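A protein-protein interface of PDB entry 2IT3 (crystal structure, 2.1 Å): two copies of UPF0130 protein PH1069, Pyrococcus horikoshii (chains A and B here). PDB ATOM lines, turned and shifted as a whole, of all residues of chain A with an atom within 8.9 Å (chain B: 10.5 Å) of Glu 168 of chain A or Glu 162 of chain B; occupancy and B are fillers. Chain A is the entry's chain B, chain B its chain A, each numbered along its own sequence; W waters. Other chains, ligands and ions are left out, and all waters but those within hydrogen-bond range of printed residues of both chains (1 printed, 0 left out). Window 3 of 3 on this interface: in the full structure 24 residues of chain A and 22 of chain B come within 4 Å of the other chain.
OE1 of Gln 98 of chain B is in hydrogen-bond range of NE1 of Trp 100 of chain B (3.1 Å). The backbone NH (N) of Phe 164 of chain B lies within hydrogen-bond range of the backbone carbonyl oxygen (O) of Leu 157 of chain B, at 2.9 Å. The side-chain amide nitrogen of Asn 160 of chain B sits at hydrogen-bond distance from the side-chain carboxylate of Glu 159 of chain B, 3.1 Å away. The side-chain amino group (NZ) of Lys 172 of chain A lies within salt-bridge range of the side-chain carboxylate (OE1) of Glu 175 of chain A, 2.5 Å away.
Glu 168 of chain A touches Phe 164 of chain B. CD1 of Tyr 169 of chain A touches CB of Phe 164 of chain B, at 3.4 Å. Tyr 169 of chain A touches Val 165 of chain B. Phe 164 of chain B touches Lys 172 of chain A. Ile 173 of chain A touches Leu 156 of chain B (CG1 to CD2, 3.9 Å). Ile 176 of chain A touches Gln 98 of chain B.
The backbone carbonyl oxygen of Leu 156 of chain B lies within hydrogen-bond range of the side-chain hydroxyl of Tyr 169 of chain A (2.5 Å). The side-chain carboxylate (OE1) of Glu 159 of chain B lies within salt-bridge range of the side-chain amino group (NZ) of Lys 172 of chain A, 2.7 Å away. OE2 of Glu 168 of chain A lies close to OE1 of Glu 162 of chain B, 2.7 Å away.
Of the 13 printed residues of chain A, 5 touch a printed residue of chain B. Hydrophobic or aromatic side chains of chain A within 4 Å of the printed part of chain B: Tyr 169, Ile 173 and Ile 176. Printed residues of chain B that touch a printed residue of chain A: Gln 98, Leu 156, Glu 159, Glu 162, Phe 164 and Val 165. Hydrophobic or aromatic side chains of chain B within 4 Å of the printed part of chain A: Leu 156, Phe 164 and Val 165. Among the printed residues, 9 pairs touch across the chains. Among the printed residues, Asp or Glu carboxylates within 4 Å of a Lys or Arg side-chain nitrogen of the other chain: Lys 172 of chain A with Glu 159 of chain B (2.7 Å).
Glu 168 of chain A touches two residues of chain B. No residue of chain B comes within 4 Å of Asn 171 of chain A. Of the printed residues of chain B, Lys 172 of chain A touches Glu 159 and Phe 164. No residue of chain A comes within 4 Å of Gly 158 of chain B. Printed residues of chain A within 4 Å of Glu 159 of chain B: Lys 172 (2.7 Å). Asn 160 of chain B touches none of the printed residues of chain A. No residue of chain A comes within 4 Å of Gly 161 of chain B. Of chain A, only Glu 168 comes within 4 Å of Glu 162 of chain B.
Water W1 bridges O of Phe 164 of chain B (2.6 Å) and N of Gly 166 of chain A (3.3 Å).
2 positions are printed for both chains. Of the 9 pairs that touch across the chains among the printed residues, none has its exchanged pair printed and touching as well.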
ATOM      1  N   LEU A  84      -8.521  26.552 -15.853  1.00  0.00           N
ATOM      2  CA  LEU A  84      -9.717  27.389 -15.795  1.00  0.00           C
ATOM      3  C   LEU A  84     -10.198  27.640 -17.238  1.00  0.00           C
ATOM      4  O   LEU A  84     -11.397  27.722 -17.514  1.00  0.00           O
ATOM      5  CB  LEU A  84      -9.380  28.726 -15.119  1.00  0.00           C
ATOM      6  CG  LEU A  84     -10.480  29.776 -14.920  1.00  0.00           C
ATOM      7  CD1 LEU A  84     -11.659  29.132 -14.203  1.00  0.00           C
ATOM      8  CD2 LEU A  84      -9.964  30.956 -14.122  1.00  0.00           C
ATOM      9  N   VAL A 165     -22.541  31.326 -11.176  1.00  0.00           N
ATOM     10  CA  VAL A 165     -21.252  31.526 -10.530  1.00  0.00           C
ATOM     11  C   VAL A 165     -20.404  32.668 -11.059  1.00  0.00           C
ATOM     12  O   VAL A 165     -20.340  32.913 -12.265  1.00  0.00           O
ATOM     13  CB  VAL A 165     -20.400  30.239 -10.582  1.00  0.00           C
ATOM     14  CG1 VAL A 165     -21.186  29.075 -10.002  1.00  0.00           C
ATOM     15  CG2 VAL A 165     -19.993  29.948 -12.007  1.00  0.00           C
ATOM     16  N   GLY A 166     -19.752  33.359 -10.128  1.00  0.00           N
ATOM     17  CA  GLY A 166     -18.877  34.457 -10.476  1.00  0.00           C
ATOM     18  C   GLY A 166     -17.499  33.897 -10.776  1.00  0.00           C
ATOM     19  O   GLY A 166     -17.306  32.673 -10.799  1.00  0.00           O
ATOM     20  N   GLU A 167     -16.539  34.787 -11.002  1.00  0.00           N
ATOM     21  CA  GLU A 167     -15.182  34.376 -11.321  1.00  0.00           C
ATOM     22  C   GLU A 167     -14.435  33.881 -10.089  1.00  0.00           C
ATOM     23  O   GLU A 167     -13.744  32.873 -10.142  1.00  0.00           O
ATOM     24  CB  GLU A 167     -14.419  35.533 -11.978  1.00  0.00           C
ATOM     25  CG  GLU A 167     -13.031  35.142 -12.473  1.00  0.00           C
ATOM     26  CD  GLU A 167     -13.047  33.871 -13.317  1.00  0.00           C
ATOM     27  OE1 GLU A 167     -13.564  33.907 -14.458  1.00  0.00           O
ATOM     28  OE2 GLU A 167     -12.549  32.829 -12.833  1.00  0.00           O
ATOM     29  N   GLU A 168     -14.572  34.587  -8.978  1.00  0.00           N
ATOM     30  CA  GLU A 168     -13.892  34.174  -7.763  1.00  0.00           C
ATOM     31  C   GLU A 168     -14.319  32.745  -7.424  1.00  0.00           C
ATOM     32  O   GLU A 168     -13.486  31.872  -7.193  1.00  0.00           O
ATOM     33  CB  GLU A 168     -14.237  35.118  -6.606  1.00  0.00           C
ATOM     34  CG  GLU A 168     -13.441  34.838  -5.332  1.00  0.00           C
ATOM     35  CD  GLU A 168     -13.809  35.758  -4.185  1.00  0.00           C
ATOM     36  OE1 GLU A 168     -14.980  35.743  -3.750  1.00  0.00           O
ATOM     37  OE2 GLU A 168     -12.929  36.503  -3.712  1.00  0.00           O
ATOM     38  N   TYR A 169     -15.628  32.518  -7.416  1.00  0.00           N
ATOM     39  CA  TYR A 169     -16.198  31.212  -7.111  1.00  0.00           C
ATOM     40  C   TYR A 169     -15.694  30.142  -8.092  1.00  0.00           C
ATOM     41  O   TYR A 169     -15.215  29.093  -7.669  1.00  0.00           O
ATOM     42  CB  TYR A 169     -17.725  31.334  -7.151  1.00  0.00           C
ATOM     43  CG  TYR A 169     -18.533  30.142  -6.685  1.00  0.00           C
ATOM     44  CD1 TYR A 169     -17.996  29.176  -5.834  1.00  0.00           C
ATOM     45  CD2 TYR A 169     -19.867  30.015  -7.061  1.00  0.00           C
ATOM     46  CE1 TYR A 169     -18.778  28.115  -5.371  1.00  0.00           C
ATOM     47  CE2 TYR A 169     -20.652  28.964  -6.608  1.00  0.00           C
ATOM     48  CZ  TYR A 169     -20.103  28.019  -5.765  1.00  0.00           C
ATOM     49  OH  TYR A 169     -20.889  26.980  -5.329  1.00  0.00           O
ATOM     50  N   LEU A 170     -15.786  30.401  -9.393  1.00  0.00           N
ATOM     51  CA  LEU A 170     -15.329  29.405 -10.354  1.00  0.00           C
ATOM     52  C   LEU A 170     -13.848  29.096 -10.121  1.00  0.00           C
ATOM     53  O   LEU A 170     -13.390  27.962 -10.203  1.00  0.00           O
ATOM     54  CB  LEU A 170     -15.523  29.987 -11.761  1.00  0.00           C
ATOM     55  CG  LEU A 170     -15.234  28.990 -12.897  1.00  0.00           C
ATOM     56  CD1 LEU A 170     -16.050  27.703 -12.792  1.00  0.00           C
ATOM     57  CD2 LEU A 170     -15.544  29.560 -14.279  1.00  0.00           C
ATOM     58  N   ASN A 171     -13.102  30.193  -9.856  1.00  0.00           N
ATOM     59  CA  ASN A 171     -11.675  30.077  -9.539  1.00  0.00           C
ATOM     60  C   ASN A 171     -11.440  28.989  -8.480  1.00  0.00           C
ATOM     61  O   ASN A 171     -10.630  28.079  -8.640  1.00  0.00           O
ATOM     62  CB  ASN A 171     -11.178  31.451  -9.039  1.00  0.00           C
ATOM     63  CG  ASN A 171      -9.852  31.823  -9.689  1.00  0.00           C
ATOM     64  OD1 ASN A 171      -9.197  30.996 -10.312  1.00  0.00           O
ATOM     65  ND2 ASN A 171      -9.440  33.118  -9.516  1.00  0.00           N
ATOM     66  N   LYS A 172     -12.174  29.116  -7.352  1.00  0.00           N
ATOM     67  CA  LYS A 172     -12.024  28.167  -6.249  1.00  0.00           C
ATOM     68  C   LYS A 172     -12.500  26.771  -6.622  1.00  0.00           C
ATOM     69  O   LYS A 172     -11.861  25.772  -6.323  1.00  0.00           O
ATOM     70  CB  LYS A 172     -12.846  28.659  -5.065  1.00  0.00           C
ATOM     71  CG  LYS A 172     -12.058  29.600  -4.157  1.00  0.00           C
ATOM     72  CD  LYS A 172     -10.750  28.994  -3.655  1.00  0.00           C
ATOM     73  CE  LYS A 172      -9.881  30.037  -2.943  1.00  0.00           C
ATOM     74  NZ  LYS A 172      -8.630  29.421  -2.505  1.00  0.00           N
ATOM     75  N   ILE A 173     -13.662  26.689  -7.263  1.00  0.00           N
ATOM     76  CA  ILE A 173     -14.209  25.397  -7.651  1.00  0.00           C
ATOM     77  C   ILE A 173     -13.156  24.573  -8.383  1.00  0.00           C
ATOM     78  O   ILE A 173     -12.939  23.403  -8.065  1.00  0.00           O
ATOM     79  CB  ILE A 173     -15.464  25.579  -8.542  1.00  0.00           C
ATOM     80  CG1 ILE A 173     -16.593  26.188  -7.697  1.00  0.00           C
ATOM     81  CG2 ILE A 173     -15.878  24.263  -9.133  1.00  0.00           C
ATOM     82  CD1 ILE A 173     -17.784  26.642  -8.482  1.00  0.00           C
ATOM     83  N   VAL A 174     -12.493  25.207  -9.345  1.00  0.00           N
ATOM     84  CA  VAL A 174     -11.456  24.564 -10.140  1.00  0.00           C
ATOM     85  C   VAL A 174     -10.248  24.205  -9.283  1.00  0.00           C
ATOM     86  O   VAL A 174      -9.695  23.121  -9.407  1.00  0.00           O
ATOM     87  CB  VAL A 174     -10.984  25.494 -11.276  1.00  0.00           C
ATOM     88  CG1 VAL A 174      -9.825  24.852 -12.022  1.00  0.00           C
ATOM     89  CG2 VAL A 174     -12.154  25.792 -12.216  1.00  0.00           C
ATOM     90  N   GLU A 175      -9.835  25.124  -8.420  1.00  0.00           N
ATOM     91  CA  GLU A 175      -8.699  24.869  -7.546  1.00  0.00           C
ATOM     92  C   GLU A 175      -8.983  23.662  -6.660  1.00  0.00           C
ATOM     93  O   GLU A 175      -8.161  22.757  -6.554  1.00  0.00           O
ATOM     94  CB  GLU A 175      -8.417  26.101  -6.688  1.00  0.00           C
ATOM     95  CG  GLU A 175      -7.482  25.865  -5.517  1.00  0.00           C
ATOM     96  CD  GLU A 175      -7.180  27.150  -4.763  1.00  0.00           C
ATOM     97  OE1 GLU A 175      -8.132  27.873  -4.407  1.00  0.00           O
ATOM     98  OE2 GLU A 175      -5.993  27.443  -4.529  1.00  0.00           O
ATOM     99  N   ILE A 176     -10.152  23.652  -6.029  1.00  0.00           N
ATOM    100  CA  ILE A 176     -10.548  22.548  -5.153  1.00  0.00           C
ATOM    101  C   ILE A 176     -10.668  21.246  -5.932  1.00  0.00           C
ATOM    102  O   ILE A 176     -10.194  20.207  -5.487  1.00  0.00           O
ATOM    103  CB  ILE A 176     -11.915  22.806  -4.479  1.00  0.00           C
ATOM    104  CG1 ILE A 176     -11.841  24.051  -3.591  1.00  0.00           C
ATOM    105  CG2 ILE A 176     -12.317  21.593  -3.657  1.00  0.00           C
ATOM    106  CD1 ILE A 176     -10.800  23.959  -2.497  1.00  0.00           C
ATOM    107  N   GLU B  62     -17.719  23.171   7.688  1.00  0.00           N
ATOM    108  CA  GLU B  62     -16.501  23.779   7.171  1.00  0.00           C
ATOM    109  C   GLU B  62     -15.309  22.867   7.415  1.00  0.00           C
ATOM    110  O   GLU B  62     -15.221  22.213   8.453  1.00  0.00           O
ATOM    111  CB  GLU B  62     -16.254  25.144   7.813  1.00  0.00           C
ATOM    112  CG  GLU B  62     -16.391  25.174   9.308  1.00  0.00           C
ATOM    113  CD  GLU B  62     -16.085  26.543   9.881  1.00  0.00           C
ATOM    114  OE1 GLU B  62     -16.448  27.557   9.242  1.00  0.00           O
ATOM    115  OE2 GLU B  62     -15.492  26.610  10.976  1.00  0.00           O
ATOM    116  N   LEU B  75     -21.833  23.139  10.994  1.00  0.00           N
ATOM    117  CA  LEU B  75     -22.554  24.359  11.347  1.00  0.00           C
ATOM    118  C   LEU B  75     -24.058  24.121  11.414  1.00  0.00           C
ATOM    119  O   LEU B  75     -24.809  24.972  11.879  1.00  0.00           O
ATOM    120  CB  LEU B  75     -22.228  25.461  10.336  1.00  0.00           C
ATOM    121  CG  LEU B  75     -20.717  25.608  10.119  1.00  0.00           C
ATOM    122  CD1 LEU B  75     -20.424  26.501   8.940  1.00  0.00           C
ATOM    123  CD2 LEU B  75     -20.076  26.147  11.381  1.00  0.00           C
ATOM    124  N   ILE B  91     -24.847  28.786   7.652  1.00  0.00           N
ATOM    125  CA  ILE B  91     -23.812  29.365   6.810  1.00  0.00           C
ATOM    126  C   ILE B  91     -23.153  30.616   7.377  1.00  0.00           C
ATOM    127  O   ILE B  91     -21.944  30.789   7.226  1.00  0.00           O
ATOM    128  CB  ILE B  91     -24.375  29.702   5.407  1.00  0.00           C
ATOM    129  CG1 ILE B  91     -24.745  28.412   4.677  1.00  0.00           C
ATOM    130  CG2 ILE B  91     -23.351  30.486   4.603  1.00  0.00           C
ATOM    131  CD1 ILE B  91     -25.440  28.641   3.342  1.00  0.00           C
ATOM    132  N   LYS B  92     -23.937  31.483   8.020  1.00  0.00           N
ATOM    133  CA  LYS B  92     -23.395  32.720   8.579  1.00  0.00           C
ATOM    134  C   LYS B  92     -22.317  32.435   9.599  1.00  0.00           C
ATOM    135  O   LYS B  92     -21.459  33.274   9.856  1.00  0.00           O
ATOM    136  CB  LYS B  92     -24.486  33.562   9.254  1.00  0.00           C
ATOM    137  CG  LYS B  92     -24.860  34.826   8.511  1.00  0.00           C
ATOM    138  CD  LYS B  92     -26.221  35.383   8.952  1.00  0.00           C
ATOM    139  CE  LYS B  92     -26.294  35.742  10.433  1.00  0.00           C
ATOM    140  NZ  LYS B  92     -27.475  36.589  10.777  1.00  0.00           N
ATOM    141  N   LYS B  93     -22.371  31.244  10.180  1.00  0.00           N
ATOM    142  CA  LYS B  93     -21.410  30.840  11.197  1.00  0.00           C
ATOM    143  C   LYS B  93     -20.066  30.421  10.612  1.00  0.00           C
ATOM    144  O   LYS B  93     -19.121  30.150  11.351  1.00  0.00           O
ATOM    145  CB  LYS B  93     -22.007  29.704  12.033  1.00  0.00           C
ATOM    146  CG  LYS B  93     -23.219  30.147  12.858  1.00  0.00           C
ATOM    147  CD  LYS B  93     -24.235  29.027  13.069  1.00  0.00           C
ATOM    148  CE  LYS B  93     -23.631  27.850  13.793  1.00  0.00           C
ATOM    149  NZ  LYS B  93     -24.590  26.711  13.903  1.00  0.00           N
ATOM    150  N   HIS B  94     -19.975  30.385   9.286  1.00  0.00           N
ATOM    151  CA  HIS B  94     -18.731  29.990   8.628  1.00  0.00           C
ATOM    152  C   HIS B  94     -17.586  30.952   8.932  1.00  0.00           C
ATOM    153  O   HIS B  94     -17.769  32.165   8.890  1.00  0.00           O
ATOM    154  CB  HIS B  94     -18.922  29.928   7.115  1.00  0.00           C
ATOM    155  CG  HIS B  94     -17.661  29.637   6.364  1.00  0.00           C
ATOM    156  ND1 HIS B  94     -16.734  28.716   6.798  1.00  0.00           N
ATOM    157  CD2 HIS B  94     -17.164  30.162   5.220  1.00  0.00           C
ATOM    158  CE1 HIS B  94     -15.717  28.687   5.954  1.00  0.00           C
ATOM    159  NE2 HIS B  94     -15.954  29.554   4.988  1.00  0.00           N
ATOM    160  N   ARG B  95     -16.406  30.404   9.216  1.00  0.00           N
ATOM    161  CA  ARG B  95     -15.234  31.224   9.513  1.00  0.00           C
ATOM    162  C   ARG B  95     -13.980  30.830   8.731  1.00  0.00           C
ATOM    163  O   ARG B  95     -13.387  31.665   8.052  1.00  0.00           O
ATOM    164  CB  ARG B  95     -14.924  31.190  11.015  1.00  0.00           C
ATOM    165  CG  ARG B  95     -16.037  31.744  11.888  1.00  0.00           C
ATOM    166  CD  ARG B  95     -16.370  33.186  11.525  1.00  0.00           C
ATOM    167  NE  ARG B  95     -17.665  33.582  12.068  1.00  0.00           N
ATOM    168  CZ  ARG B  95     -18.286  34.718  11.774  1.00  0.00           C
ATOM    169  NH1 ARG B  95     -17.730  35.588  10.935  1.00  0.00           N
ATOM    170  NH2 ARG B  95     -19.472  34.979  12.311  1.00  0.00           N
ATOM    171  N   SER B  96     -13.582  29.564   8.811  1.00  0.00           N
ATOM    172  CA  SER B  96     -12.377  29.118   8.122  1.00  0.00           C
ATOM    173  C   SER B  96     -12.543  27.831   7.335  1.00  0.00           C
ATOM    174  O   SER B  96     -13.501  27.082   7.524  1.00  0.00           O
ATOM    175  CB  SER B  96     -11.237  28.931   9.119  1.00  0.00           C
ATOM    176  OG  SER B  96     -11.521  27.865  10.014  1.00  0.00           O
ATOM    177  N   GLY B  97     -11.578  27.574   6.462  1.00  0.00           N
ATOM    178  CA  GLY B  97     -11.630  26.378   5.648  1.00  0.00           C
ATOM    179  C   GLY B  97     -12.663  26.480   4.543  1.00  0.00           C
ATOM    180  O   GLY B  97     -13.177  27.555   4.229  1.00  0.00           O
ATOM    181  N   GLN B  98     -12.972  25.342   3.948  1.00  0.00           N
ATOM    182  CA  GLN B  98     -13.944  25.294   2.875  1.00  0.00           C
ATOM    183  C   GLN B  98     -15.326  25.064   3.465  1.00  0.00           C
ATOM    184  O   GLN B  98     -15.488  24.302   4.415  1.00  0.00           O
ATOM    185  CB  GLN B  98     -13.596  24.154   1.931  1.00  0.00           C
ATOM    186  CG  GLN B  98     -12.100  23.967   1.763  1.00  0.00           C
ATOM    187  CD  GLN B  98     -11.773  22.692   1.026  1.00  0.00           C
ATOM    188  OE1 GLN B  98     -12.416  21.654   1.237  1.00  0.00           O
ATOM    189  NE2 GLN B  98     -10.764  22.754   0.164  1.00  0.00           N
ATOM    190  N   LEU B  99     -16.319  25.731   2.897  1.00  0.00           N
ATOM    191  CA  LEU B  99     -17.684  25.593   3.353  1.00  0.00           C
ATOM    192  C   LEU B  99     -18.422  24.692   2.393  1.00  0.00           C
ATOM    193  O   LEU B  99     -18.448  24.956   1.184  1.00  0.00           O
ATOM    194  CB  LEU B  99     -18.372  26.960   3.401  1.00  0.00           C
ATOM    195  CG  LEU B  99     -19.856  26.943   3.761  1.00  0.00           C
ATOM    196  CD1 LEU B  99     -20.061  26.332   5.152  1.00  0.00           C
ATOM    197  CD2 LEU B  99     -20.384  28.365   3.704  1.00  0.00           C
ATOM    198  N   TRP B 100     -19.036  23.648   2.946  1.00  0.00           N
ATOM    199  CA  TRP B 100     -19.784  22.657   2.176  1.00  0.00           C
ATOM    200  C   TRP B 100     -21.217  22.449   2.633  1.00  0.00           C
ATOM    201  O   TRP B 100     -21.511  22.463   3.823  1.00  0.00           O
ATOM    202  CB  TRP B 100     -19.122  21.273   2.261  1.00  0.00           C
ATOM    203  CG  TRP B 100     -17.727  21.201   1.752  1.00  0.00           C
ATOM    204  CD1 TRP B 100     -16.592  21.561   2.417  1.00  0.00           C
ATOM    205  CD2 TRP B 100     -17.319  20.800   0.436  1.00  0.00           C
ATOM    206  NE1 TRP B 100     -15.502  21.417   1.591  1.00  0.00           N
ATOM    207  CE2 TRP B 100     -15.919  20.952   0.371  1.00  0.00           C
ATOM    208  CE3 TRP B 100     -18.002  20.330  -0.695  1.00  0.00           C
ATOM    209  CZ2 TRP B 100     -15.179  20.651  -0.789  1.00  0.00           C
ATOM    210  CZ3 TRP B 100     -17.269  20.030  -1.849  1.00  0.00           C
ATOM    211  CH2 TRP B 100     -15.875  20.194  -1.885  1.00  0.00           C
ATOM    212  N   VAL B 155     -21.854  20.212  -2.138  1.00  0.00           N
ATOM    213  CA  VAL B 155     -21.787  21.552  -2.711  1.00  0.00           C
ATOM    214  C   VAL B 155     -20.833  22.520  -2.022  1.00  0.00           C
ATOM    215  O   VAL B 155     -20.991  22.826  -0.842  1.00  0.00           O
ATOM    216  CB  VAL B 155     -23.188  22.203  -2.734  1.00  0.00           C
ATOM    217  CG1 VAL B 155     -23.124  23.544  -3.448  1.00  0.00           C
ATOM    218  CG2 VAL B 155     -24.190  21.277  -3.416  1.00  0.00           C
ATOM    219  N   LEU B 156     -19.838  22.998  -2.768  1.00  0.00           N
ATOM    220  CA  LEU B 156     -18.870  23.968  -2.247  1.00  0.00           C
ATOM    221  C   LEU B 156     -19.565  25.324  -2.285  1.00  0.00           C
ATOM    222  O   LEU B 156     -19.984  25.759  -3.347  1.00  0.00           O
ATOM    223  CB  LEU B 156     -17.629  24.023  -3.139  1.00  0.00           C
ATOM    224  CG  LEU B 156     -16.594  25.098  -2.790  1.00  0.00           C
ATOM    225  CD1 LEU B 156     -15.769  24.661  -1.564  1.00  0.00           C
ATOM    226  CD2 LEU B 156     -15.682  25.321  -3.998  1.00  0.00           C
ATOM    227  N   LEU B 157     -19.691  25.989  -1.139  1.00  0.00           N
ATOM    228  CA  LEU B 157     -20.376  27.287  -1.104  1.00  0.00           C
ATOM    229  C   LEU B 157     -19.490  28.464  -0.746  1.00  0.00           C
ATOM    230  O   LEU B 157     -19.883  29.616  -0.936  1.00  0.00           O
ATOM    231  CB  LEU B 157     -21.543  27.245  -0.122  1.00  0.00           C
ATOM    232  CG  LEU B 157     -22.620  26.200  -0.404  1.00  0.00           C
ATOM    233  CD1 LEU B 157     -23.622  26.215   0.736  1.00  0.00           C
ATOM    234  CD2 LEU B 157     -23.293  26.492  -1.740  1.00  0.00           C
ATOM    235  N   GLY B 158     -18.305  28.183  -0.219  1.00  0.00           N
ATOM    236  CA  GLY B 158     -17.417  29.261   0.153  1.00  0.00           C
ATOM    237  C   GLY B 158     -16.115  28.778   0.737  1.00  0.00           C
ATOM    238  O   GLY B 158     -15.901  27.572   0.903  1.00  0.00           O
ATOM    239  N   GLU B 159     -15.227  29.720   1.030  1.00  0.00           N
ATOM    240  CA  GLU B 159     -13.948  29.381   1.626  1.00  0.00           C
ATOM    241  C   GLU B 159     -13.432  30.519   2.483  1.00  0.00           C
ATOM    242  O   GLU B 159     -13.673  31.692   2.197  1.00  0.00           O
ATOM    243  CB  GLU B 159     -12.897  29.039   0.562  1.00  0.00           C
ATOM    244  CG  GLU B 159     -11.652  28.387   1.174  1.00  0.00           C
ATOM    245  CD  GLU B 159     -10.468  28.328   0.232  1.00  0.00           C
ATOM    246  OE1 GLU B 159      -9.942  29.402  -0.132  1.00  0.00           O
ATOM    247  OE2 GLU B 159     -10.053  27.210  -0.139  1.00  0.00           O
ATOM    248  N   ASN B 160     -12.717  30.150   3.541  1.00  0.00           N
ATOM    249  CA  ASN B 160     -12.135  31.105   4.469  1.00  0.00           C
ATOM    250  C   ASN B 160     -13.040  32.267   4.860  1.00  0.00           C
ATOM    251  O   ASN B 160     -12.617  33.424   4.861  1.00  0.00           O
ATOM    252  CB  ASN B 160     -10.816  31.635   3.908  1.00  0.00           C
ATOM    253  CG  ASN B 160      -9.772  30.547   3.776  1.00  0.00           C
ATOM    254  OD1 ASN B 160      -9.544  29.767   4.710  1.00  0.00           O
ATOM    255  ND2 ASN B 160      -9.124  30.486   2.615  1.00  0.00           N
ATOM    256  N   GLY B 161     -14.285  31.949   5.199  1.00  0.00           N
ATOM    257  CA  GLY B 161     -15.220  32.973   5.621  1.00  0.00           C
ATOM    258  C   GLY B 161     -15.992  33.655   4.515  1.00  0.00           C
ATOM    259  O   GLY B 161     -17.037  34.248   4.768  1.00  0.00           O
ATOM    260  N   GLU B 162     -15.489  33.580   3.289  1.00  0.00           N
ATOM    261  CA  GLU B 162     -16.173  34.212   2.165  1.00  0.00           C
ATOM    262  C   GLU B 162     -17.232  33.310   1.547  1.00  0.00           C
ATOM    263  O   GLU B 162     -16.925  32.225   1.061  1.00  0.00           O
ATOM    264  CB  GLU B 162     -15.160  34.625   1.087  1.00  0.00           C
ATOM    265  CG  GLU B 162     -15.814  35.135  -0.192  1.00  0.00           C
ATOM    266  CD  GLU B 162     -14.907  36.043  -1.006  1.00  0.00           C
ATOM    267  OE1 GLU B 162     -13.770  35.630  -1.334  1.00  0.00           O
ATOM    268  OE2 GLU B 162     -15.345  37.174  -1.322  1.00  0.00           O
ATOM    269  N   ILE B 163     -18.481  33.766   1.566  1.00  0.00           N
ATOM    270  CA  ILE B 163     -19.585  33.006   0.991  1.00  0.00           C
ATOM    271  C   ILE B 163     -19.691  33.387  -0.483  1.00  0.00           C
ATOM    272  O   ILE B 163     -19.956  34.545  -0.818  1.00  0.00           O
ATOM    273  CB  ILE B 163     -20.919  33.331   1.699  1.00  0.00           C
ATOM    274  CG1 ILE B 163     -20.734  33.264   3.217  1.00  0.00           C
ATOM    275  CG2 ILE B 163     -21.998  32.352   1.261  1.00  0.00           C
ATOM    276  CD1 ILE B 163     -20.098  31.979   3.709  1.00  0.00           C
ATOM    277  N   PHE B 164     -19.487  32.413  -1.362  1.00  0.00           N
ATOM    278  CA  PHE B 164     -19.534  32.680  -2.793  1.00  0.00           C
ATOM    279  C   PHE B 164     -20.929  32.771  -3.391  1.00  0.00           C
ATOM    280  O   PHE B 164     -21.086  33.232  -4.518  1.00  0.00           O
ATOM    281  CB  PHE B 164     -18.736  31.619  -3.556  1.00  0.00           C
ATOM    282  CG  PHE B 164     -17.270  31.603  -3.223  1.00  0.00           C
ATOM    283  CD1 PHE B 164     -16.506  32.762  -3.321  1.00  0.00           C
ATOM    284  CD2 PHE B 164     -16.648  30.426  -2.824  1.00  0.00           C
ATOM    285  CE1 PHE B 164     -15.146  32.749  -3.027  1.00  0.00           C
ATOM    286  CE2 PHE B 164     -15.284  30.399  -2.528  1.00  0.00           C
ATOM    287  CZ  PHE B 164     -14.532  31.566  -2.630  1.00  0.00           C
ATOM    288  N   VAL B 165     -21.946  32.349  -2.654  1.00  0.00           N
ATOM    289  CA  VAL B 165     -23.296  32.389  -3.194  1.00  0.00           C
ATOM    290  C   VAL B 165     -24.258  33.281  -2.432  1.00  0.00           C
ATOM    291  O   VAL B 165     -24.036  33.610  -1.272  1.00  0.00           O
ATOM    292  CB  VAL B 165     -23.895  30.981  -3.257  1.00  0.00           C
ATOM    293  CG1 VAL B 165     -23.000  30.087  -4.113  1.00  0.00           C
ATOM    294  CG2 VAL B 165     -24.047  30.417  -1.854  1.00  0.00           C
ATOM    295  N   GLY B 166     -25.330  33.668  -3.112  1.00  0.00           N
ATOM    296  CA  GLY B 166     -26.336  34.513  -2.505  1.00  0.00           C
ATOM    297  C   GLY B 166     -27.565  33.711  -2.122  1.00  0.00           C
ATOM    298  O   GLY B 166     -27.613  32.492  -2.299  1.00  0.00           O
HETATM  299  O   HOH W   1     -20.900  33.591  -7.036  1.00  0.00           O
